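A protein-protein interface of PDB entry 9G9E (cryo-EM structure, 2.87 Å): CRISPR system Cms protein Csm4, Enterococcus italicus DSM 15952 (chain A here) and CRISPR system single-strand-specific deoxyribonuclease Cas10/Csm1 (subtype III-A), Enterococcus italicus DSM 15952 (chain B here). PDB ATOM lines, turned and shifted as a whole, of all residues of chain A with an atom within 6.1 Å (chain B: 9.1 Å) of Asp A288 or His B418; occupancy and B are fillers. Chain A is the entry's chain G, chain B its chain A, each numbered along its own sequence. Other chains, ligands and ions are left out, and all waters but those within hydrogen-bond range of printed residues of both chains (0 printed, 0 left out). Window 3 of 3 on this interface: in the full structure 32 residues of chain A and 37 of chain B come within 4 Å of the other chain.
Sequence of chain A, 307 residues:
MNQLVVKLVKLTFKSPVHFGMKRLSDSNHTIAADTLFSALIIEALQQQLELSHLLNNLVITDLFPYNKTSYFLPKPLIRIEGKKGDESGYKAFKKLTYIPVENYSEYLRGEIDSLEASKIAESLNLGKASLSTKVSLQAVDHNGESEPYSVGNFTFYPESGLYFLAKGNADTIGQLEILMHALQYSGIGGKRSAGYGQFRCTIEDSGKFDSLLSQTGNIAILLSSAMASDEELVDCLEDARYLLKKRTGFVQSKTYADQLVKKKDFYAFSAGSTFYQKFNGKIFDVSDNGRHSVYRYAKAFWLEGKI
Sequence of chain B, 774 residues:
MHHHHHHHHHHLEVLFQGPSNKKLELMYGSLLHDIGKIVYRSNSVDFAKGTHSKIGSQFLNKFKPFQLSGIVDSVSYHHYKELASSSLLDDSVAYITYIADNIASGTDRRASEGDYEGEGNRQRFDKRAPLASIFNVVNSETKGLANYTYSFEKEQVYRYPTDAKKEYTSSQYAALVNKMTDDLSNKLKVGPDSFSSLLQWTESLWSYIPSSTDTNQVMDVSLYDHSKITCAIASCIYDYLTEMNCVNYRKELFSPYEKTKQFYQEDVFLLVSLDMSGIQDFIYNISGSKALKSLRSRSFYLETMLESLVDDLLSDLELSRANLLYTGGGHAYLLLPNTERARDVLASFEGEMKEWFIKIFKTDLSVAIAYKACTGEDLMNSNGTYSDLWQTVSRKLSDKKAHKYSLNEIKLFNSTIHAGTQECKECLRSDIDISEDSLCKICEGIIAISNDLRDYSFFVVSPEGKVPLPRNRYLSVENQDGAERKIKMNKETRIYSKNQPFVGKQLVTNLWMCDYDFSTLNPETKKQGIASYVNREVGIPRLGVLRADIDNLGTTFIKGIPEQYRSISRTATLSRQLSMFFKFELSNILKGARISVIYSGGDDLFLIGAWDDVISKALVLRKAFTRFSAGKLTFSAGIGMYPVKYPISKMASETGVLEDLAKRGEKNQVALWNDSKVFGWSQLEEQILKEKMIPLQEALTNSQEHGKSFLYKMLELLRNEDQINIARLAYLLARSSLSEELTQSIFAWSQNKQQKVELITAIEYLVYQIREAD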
ATOM      1  N   TYR A 256      14.241  -3.029 -22.248  1.00  0.00           N
ATOM      2  CA  TYR A 256      13.377  -1.865 -22.071  1.00  0.00           C
ATOM      3  C   TYR A 256      14.133  -0.696 -21.454  1.00  0.00           C
ATOM      4  O   TYR A 256      13.981   0.451 -21.893  1.00  0.00           O
ATOM      5  CB  TYR A 256      12.169  -2.235 -21.213  1.00  0.00           C
ATOM      6  CG  TYR A 256      11.130  -1.142 -21.109  1.00  0.00           C
ATOM      7  CD1 TYR A 256      10.386  -0.753 -22.214  1.00  0.00           C
ATOM      8  CD2 TYR A 256      10.889  -0.501 -19.900  1.00  0.00           C
ATOM      9  CE1 TYR A 256       9.436   0.244 -22.120  1.00  0.00           C
ATOM     10  CE2 TYR A 256       9.943   0.496 -19.799  1.00  0.00           C
ATOM     11  CZ  TYR A 256       9.219   0.866 -20.909  1.00  0.00           C
ATOM     12  OH  TYR A 256       8.275   1.860 -20.807  1.00  0.00           O
ATOM     13  N   LYS A 262       8.112   0.013 -13.742  1.00  0.00           N
ATOM     14  CA  LYS A 262       6.713  -0.308 -13.966  1.00  0.00           C
ATOM     15  C   LYS A 262       6.226   0.306 -15.275  1.00  0.00           C
ATOM     16  O   LYS A 262       6.827   1.235 -15.821  1.00  0.00           O
ATOM     17  CB  LYS A 262       5.850   0.194 -12.808  1.00  0.00           C
ATOM     18  CG  LYS A 262       6.277  -0.311 -11.443  1.00  0.00           C
ATOM     19  CD  LYS A 262       5.312   0.134 -10.357  1.00  0.00           C
ATOM     20  CE  LYS A 262       3.959  -0.544 -10.503  1.00  0.00           C
ATOM     21  NZ  LYS A 262       3.001  -0.109  -9.450  1.00  0.00           N
ATOM     22  N   LYS A 263       5.120  -0.230 -15.777  1.00  0.00           N
ATOM     23  CA  LYS A 263       4.442   0.336 -16.932  1.00  0.00           C
ATOM     24  C   LYS A 263       3.268   1.193 -16.474  1.00  0.00           C
ATOM     25  O   LYS A 263       2.847   1.143 -15.315  1.00  0.00           O
ATOM     26  CB  LYS A 263       3.958  -0.761 -17.887  1.00  0.00           C
ATOM     27  CG  LYS A 263       3.535  -2.058 -17.219  1.00  0.00           C
ATOM     28  CD  LYS A 263       3.095  -3.073 -18.265  1.00  0.00           C
ATOM     29  CE  LYS A 263       2.557  -4.346 -17.631  1.00  0.00           C
ATOM     30  NZ  LYS A 263       3.639  -5.285 -17.237  1.00  0.00           N
ATOM     31  N   LYS A 264       2.747   1.992 -17.402  1.00  0.00           N
ATOM     32  CA  LYS A 264       1.675   2.921 -17.071  1.00  0.00           C
ATOM     33  C   LYS A 264       0.430   2.171 -16.615  1.00  0.00           C
ATOM     34  O   LYS A 264       0.114   1.088 -17.115  1.00  0.00           O
ATOM     35  CB  LYS A 264       1.347   3.805 -18.274  1.00  0.00           C
ATOM     36  CG  LYS A 264       2.500   4.679 -18.734  1.00  0.00           C
ATOM     37  CD  LYS A 264       2.044   5.690 -19.773  1.00  0.00           C
ATOM     38  CE  LYS A 264       1.380   5.003 -20.953  1.00  0.00           C
ATOM     39  NZ  LYS A 264       1.135   5.942 -22.080  1.00  0.00           N
ATOM     40  N   ASP A 265      -0.269   2.756 -15.645  1.00  0.00           N
ATOM     41  CA  ASP A 265      -1.476   2.152 -15.099  1.00  0.00           C
ATOM     42  C   ASP A 265      -2.536   1.999 -16.182  1.00  0.00           C
ATOM     43  O   ASP A 265      -2.767   2.913 -16.977  1.00  0.00           O
ATOM     44  CB  ASP A 265      -2.021   3.010 -13.959  1.00  0.00           C
ATOM     45  CG  ASP A 265      -1.521   2.566 -12.607  1.00  0.00           C
ATOM     46  OD1 ASP A 265      -1.394   1.346 -12.396  1.00  0.00           O
ATOM     47  OD2 ASP A 265      -1.238   3.437 -11.757  1.00  0.00           O
ATOM     48  N   ASP A 285      -0.729   1.113 -25.612  1.00  0.00           N
ATOM     49  CA  ASP A 285       0.679   1.220 -25.255  1.00  0.00           C
ATOM     50  C   ASP A 285       0.784   1.744 -23.829  1.00  0.00           C
ATOM     51  O   ASP A 285       0.286   2.832 -23.524  1.00  0.00           O
ATOM     52  CB  ASP A 285       1.419   2.140 -26.225  1.00  0.00           C
ATOM     53  CG  ASP A 285       2.897   2.247 -25.912  1.00  0.00           C
ATOM     54  OD1 ASP A 285       3.545   1.195 -25.731  1.00  0.00           O
ATOM     55  OD2 ASP A 285       3.411   3.382 -25.852  1.00  0.00           O
ATOM     56  N   VAL A 286       1.431   0.968 -22.961  1.00  0.00           N
ATOM     57  CA  VAL A 286       1.612   1.356 -21.568  1.00  0.00           C
ATOM     58  C   VAL A 286       3.090   1.623 -21.321  1.00  0.00           C
ATOM     59  O   VAL A 286       3.584   1.470 -20.199  1.00  0.00           O
ATOM     60  CB  VAL A 286       1.070   0.280 -20.611  1.00  0.00           C
ATOM     61  CG1 VAL A 286      -0.447   0.328 -20.573  1.00  0.00           C
ATOM     62  CG2 VAL A 286       1.547  -1.092 -21.043  1.00  0.00           C
ATOM     63  N   SER A 287       3.802   2.021 -22.371  1.00  0.00           N
ATOM     64  CA  SER A 287       5.222   2.320 -22.276  1.00  0.00           C
ATOM     65  C   SER A 287       5.426   3.807 -22.020  1.00  0.00           C
ATOM     66  O   SER A 287       4.716   4.650 -22.575  1.00  0.00           O
ATOM     67  CB  SER A 287       5.945   1.902 -23.557  1.00  0.00           C
ATOM     68  OG  SER A 287       7.331   2.179 -23.485  1.00  0.00           O
ATOM     69  N   ASP A 288       6.398   4.122 -21.167  1.00  0.00           N
ATOM     70  CA  ASP A 288       6.727   5.502 -20.817  1.00  0.00           C
ATOM     71  C   ASP A 288       8.159   5.724 -21.293  1.00  0.00           C
ATOM     72  O   ASP A 288       9.120   5.496 -20.554  1.00  0.00           O
ATOM     73  CB  ASP A 288       6.545   5.747 -19.255  1.00  0.00           C
ATOM     74  CG  ASP A 288       7.312   6.968 -18.721  1.00  0.00           C
ATOM     75  OD1 ASP A 288       7.938   7.729 -19.485  1.00  0.00           O
ATOM     76  OD2 ASP A 288       7.217   7.214 -17.502  1.00  0.00           O
ATOM     77  N   ASN A 289       8.294   6.149 -22.549  1.00  0.00           N
ATOM     78  CA  ASN A 289       9.573   6.580 -23.118  1.00  0.00           C
ATOM     79  C   ASN A 289      10.648   5.499 -22.998  1.00  0.00           C
ATOM     80  O   ASN A 289      11.820   5.788 -22.749  1.00  0.00           O
ATOM     81  CB  ASN A 289      10.040   7.886 -22.473  1.00  0.00           C
ATOM     82  CG  ASN A 289       9.077   9.029 -22.723  1.00  0.00           C
ATOM     83  OD1 ASN A 289       8.565   9.647 -21.787  1.00  0.00           O
ATOM     84  ND2 ASN A 289       8.820   9.314 -23.993  1.00  0.00           N
ATOM     85  N   GLY A 290      10.246   4.239 -23.177  1.00  0.00           N
ATOM     86  CA  GLY A 290      11.178   3.134 -23.145  1.00  0.00           C
ATOM     87  C   GLY A 290      11.808   2.873 -24.501  1.00  0.00           C
ATOM     88  O   GLY A 290      11.517   3.532 -25.497  1.00  0.00           O
ATOM     89  N   ASN B 414      -7.615   6.151 -18.012  1.00  0.00           N
ATOM     90  CA  ASN B 414      -6.639   5.617 -18.953  1.00  0.00           C
ATOM     91  C   ASN B 414      -5.657   6.665 -19.461  1.00  0.00           C
ATOM     92  O   ASN B 414      -4.691   6.304 -20.139  1.00  0.00           O
ATOM     93  CB  ASN B 414      -7.352   4.966 -20.139  1.00  0.00           C
ATOM     94  CG  ASN B 414      -7.987   3.638 -19.779  1.00  0.00           C
ATOM     95  OD1 ASN B 414      -7.516   2.935 -18.885  1.00  0.00           O
ATOM     96  ND2 ASN B 414      -9.061   3.287 -20.475  1.00  0.00           N
ATOM     97  N   SER B 415      -5.875   7.945 -19.155  1.00  0.00           N
ATOM     98  CA  SER B 415      -4.979   9.017 -19.593  1.00  0.00           C
ATOM     99  C   SER B 415      -3.850   9.167 -18.577  1.00  0.00           C
ATOM    100  O   SER B 415      -3.839  10.064 -17.730  1.00  0.00           O
ATOM    101  CB  SER B 415      -5.745  10.320 -19.778  1.00  0.00           C
ATOM    102  OG  SER B 415      -6.664  10.224 -20.851  1.00  0.00           O
ATOM    103  N   THR B 416      -2.880   8.262 -18.669  1.00  0.00           N
ATOM    104  CA  THR B 416      -1.697   8.293 -17.822  1.00  0.00           C
ATOM    105  C   THR B 416      -0.503   8.792 -18.625  1.00  0.00           C
ATOM    106  O   THR B 416      -0.271   8.349 -19.753  1.00  0.00           O
ATOM    107  CB  THR B 416      -1.400   6.905 -17.246  1.00  0.00           C
ATOM    108  OG1 THR B 416      -2.578   6.384 -16.619  1.00  0.00           O
ATOM    109  CG2 THR B 416      -0.283   6.982 -16.219  1.00  0.00           C
ATOM    110  N   ILE B 417       0.252   9.716 -18.037  1.00  0.00           N
ATOM    111  CA  ILE B 417       1.382  10.340 -18.711  1.00  0.00           C
ATOM    112  C   ILE B 417       2.704   9.697 -18.312  1.00  0.00           C
ATOM    113  O   ILE B 417       3.540   9.412 -19.169  1.00  0.00           O
ATOM    114  CB  ILE B 417       1.398  11.859 -18.431  1.00  0.00           C
ATOM    115  CG1 ILE B 417       0.042  12.481 -18.768  1.00  0.00           C
ATOM    116  CG2 ILE B 417       2.510  12.535 -19.220  1.00  0.00           C
ATOM    117  CD1 ILE B 417       0.010  13.986 -18.632  1.00  0.00           C
ATOM    118  N   HIS B 418       2.907   9.458 -17.020  1.00  0.00           N
ATOM    119  CA  HIS B 418       4.155   8.912 -16.506  1.00  0.00           C
ATOM    120  C   HIS B 418       3.902   7.563 -15.848  1.00  0.00           C
ATOM    121  O   HIS B 418       2.830   7.327 -15.283  1.00  0.00           O
ATOM    122  CB  HIS B 418       4.809   9.871 -15.505  1.00  0.00           C
ATOM    123  CG  HIS B 418       5.293  11.146 -16.120  1.00  0.00           C
ATOM    124  ND1 HIS B 418       5.089  12.379 -15.539  1.00  0.00           N
ATOM    125  CD2 HIS B 418       5.975  11.380 -17.267  1.00  0.00           C
ATOM    126  CE1 HIS B 418       5.623  13.317 -16.301  1.00  0.00           C
ATOM    127  NE2 HIS B 418       6.167  12.737 -17.356  1.00  0.00           N
ATOM    128  N   ALA B 419       4.898   6.685 -15.927  1.00  0.00           N
ATOM    129  CA  ALA B 419       4.780   5.338 -15.391  1.00  0.00           C
ATOM    130  C   ALA B 419       4.784   5.369 -13.863  1.00  0.00           C
ATOM    131  O   ALA B 419       4.849   6.426 -13.228  1.00  0.00           O
ATOM    132  CB  ALA B 419       5.908   4.457 -15.921  1.00  0.00           C
ATOM    133  N   GLY B 420       4.710   4.177 -13.269  1.00  0.00           N
ATOM    134  CA  GLY B 420       4.644   4.086 -11.820  1.00  0.00           C
ATOM    135  C   GLY B 420       5.909   4.562 -11.133  1.00  0.00           C
ATOM    136  O   GLY B 420       5.845   5.245 -10.108  1.00  0.00           O
ATOM    137  N   THR B 421       7.071   4.207 -11.686  1.00  0.00           N
ATOM    138  CA  THR B 421       8.390   4.521 -11.120  1.00  0.00           C
ATOM    139  C   THR B 421       8.403   4.058  -9.666  1.00  0.00           C
ATOM    140  O   THR B 421       8.197   2.855  -9.425  1.00  0.00           O
ATOM    141  CB  THR B 421       8.718   5.999 -11.369  1.00  0.00           C
ATOM    142  OG1 THR B 421       7.933   6.840 -10.515  1.00  0.00           O
ATOM    143  CG2 THR B 421       8.448   6.368 -12.820  1.00  0.00           C
ATOM    144  N   GLN B 422       8.637   4.929  -8.688  1.00  0.00           N
ATOM    145  CA  GLN B 422       8.620   4.511  -7.294  1.00  0.00           C
ATOM    146  C   GLN B 422       7.199   4.182  -6.848  1.00  0.00           C
ATOM    147  O   GLN B 422       6.224   4.785  -7.302  1.00  0.00           O
ATOM    148  CB  GLN B 422       9.207   5.604  -6.400  1.00  0.00           C
ATOM    149  CG  GLN B 422       9.669   5.112  -5.038  1.00  0.00           C
ATOM    150  CD  GLN B 422      10.259   6.219  -4.186  1.00  0.00           C
ATOM    151  OE1 GLN B 422      10.289   7.381  -4.592  1.00  0.00           O
ATOM    152  NE2 GLN B 422      10.728   5.863  -2.996  1.00  0.00           N
ATOM    153  N   SER B 430       1.423   3.609  -6.968  1.00  0.00           N
ATOM    154  CA  SER B 430       2.468   4.369  -7.633  1.00  0.00           C
ATOM    155  C   SER B 430       1.979   5.615  -8.357  1.00  0.00           C
ATOM    156  O   SER B 430       2.799   6.493  -8.647  1.00  0.00           O
ATOM    157  CB  SER B 430       3.213   3.475  -8.635  1.00  0.00           C
ATOM    158  OG  SER B 430       2.386   3.156  -9.739  1.00  0.00           O
ATOM    159  N   ASP B 431       0.682   5.724  -8.662  1.00  0.00           N
ATOM    160  CA  ASP B 431       0.190   6.926  -9.329  1.00  0.00           C
ATOM    161  C   ASP B 431       0.282   8.141  -8.413  1.00  0.00           C
ATOM    162  O   ASP B 431       0.550   9.255  -8.875  1.00  0.00           O
ATOM    163  CB  ASP B 431      -1.244   6.714  -9.820  1.00  0.00           C
ATOM    164  CG  ASP B 431      -2.088   5.917  -8.844  1.00  0.00           C
ATOM    165  OD1 ASP B 431      -2.084   6.243  -7.640  1.00  0.00           O
ATOM    166  OD2 ASP B 431      -2.767   4.966  -9.285  1.00  0.00           O
ATOM    167  N   ILE B 432       0.168   7.890  -7.104  1.00  0.00           N
ATOM    168  CA  ILE B 432       0.309   8.975  -6.088  1.00  0.00           C
ATOM    169  C   ILE B 432       1.809   9.259  -5.895  1.00  0.00           C
ATOM    170  O   ILE B 432       2.624   8.347  -6.153  1.00  0.00           O
ATOM    171  CB  ILE B 432      -0.370   8.535  -4.777  1.00  0.00           C
ATOM    172  CG1 ILE B 432      -0.328   9.624  -3.702  1.00  0.00           C
ATOM    173  CG2 ILE B 432       0.222   7.219  -4.270  1.00  0.00           C
ATOM    174  CD1 ILE B 432      -0.968   9.216  -2.387  1.00  0.00           C
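The side-chain hydroxyl (OG1) of Thr B416 lies within hydrogen-bond range of the backbone carbonyl oxygen (O) of Asp A265, 3.5 Å away.
N of Ala B419 is in hydrogen-bond range of OD2 of Asp A288 (2.9 Å).
The side-chain hydroxyl (OG) of Ser B430 is in hydrogen-bond range of the side-chain amino group (NZ) of Lys A262 (3.3 Å).
The side-chain carboxylate of Asp A265 lies close to the side-chain carboxylate of Asp B431, 3.3 Å away.
The side-chain hydroxyl (OH) of Tyr A256 is in hydrogen-bond range of the backbone NH (N) of Asp A288 (3.0 Å).
O of Val A286 lies within hydrogen-bond range of N of Lys A264, 3.0 Å away.
The side-chain carboxylate (OD1) of Asp A288 lies close to the side-chain amide oxygen (OD1) of Asn A289, 3.1 Å away.
CB of Ala B419 touches O of Lys A262, at 3.4 Å.
CD of Lys A264 touches O of Thr B416, at 3.5 Å.
Asp A288 touches His B418 (OD2 to CA, 3.6 Å).
Of the printed residues of chain B, Lys A262 touches Ala B419 (3.4 Å) and Ser B430 (3.3 Å).
Of the printed residues of chain B, Lys A264 touches Thr B416.
Of the printed residues of chain B, Asp A265 touches Thr B416 (3.5 Å) and Asp B431 (3.3 Å).
No residue of chain B comes within 4 Å of Ser A287.
Asp A288 touches two residues of chain B.
His B418 touches just one residue of chain A: Asp A288 (3.6 Å).
Thr B421 touches none of the printed residues of chain A.
The nearest residue of chain B that does not touch Asp A288 is Ile B417 (4.5 Å).
The nearest residue of chain A that does not touch His B418 is Lys A264 (4.3 Å).
The nearest printed residue of chain B that does not touch Lys A264 is Ile B417 (4.1 Å).
Of the 11 printed residues of chain A, 4 touch a printed residue of chain B.
Printed residues of chain A that touch a printed residue of chain B: Lys A262, Lys A264, Asp A265 and Asp A288.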
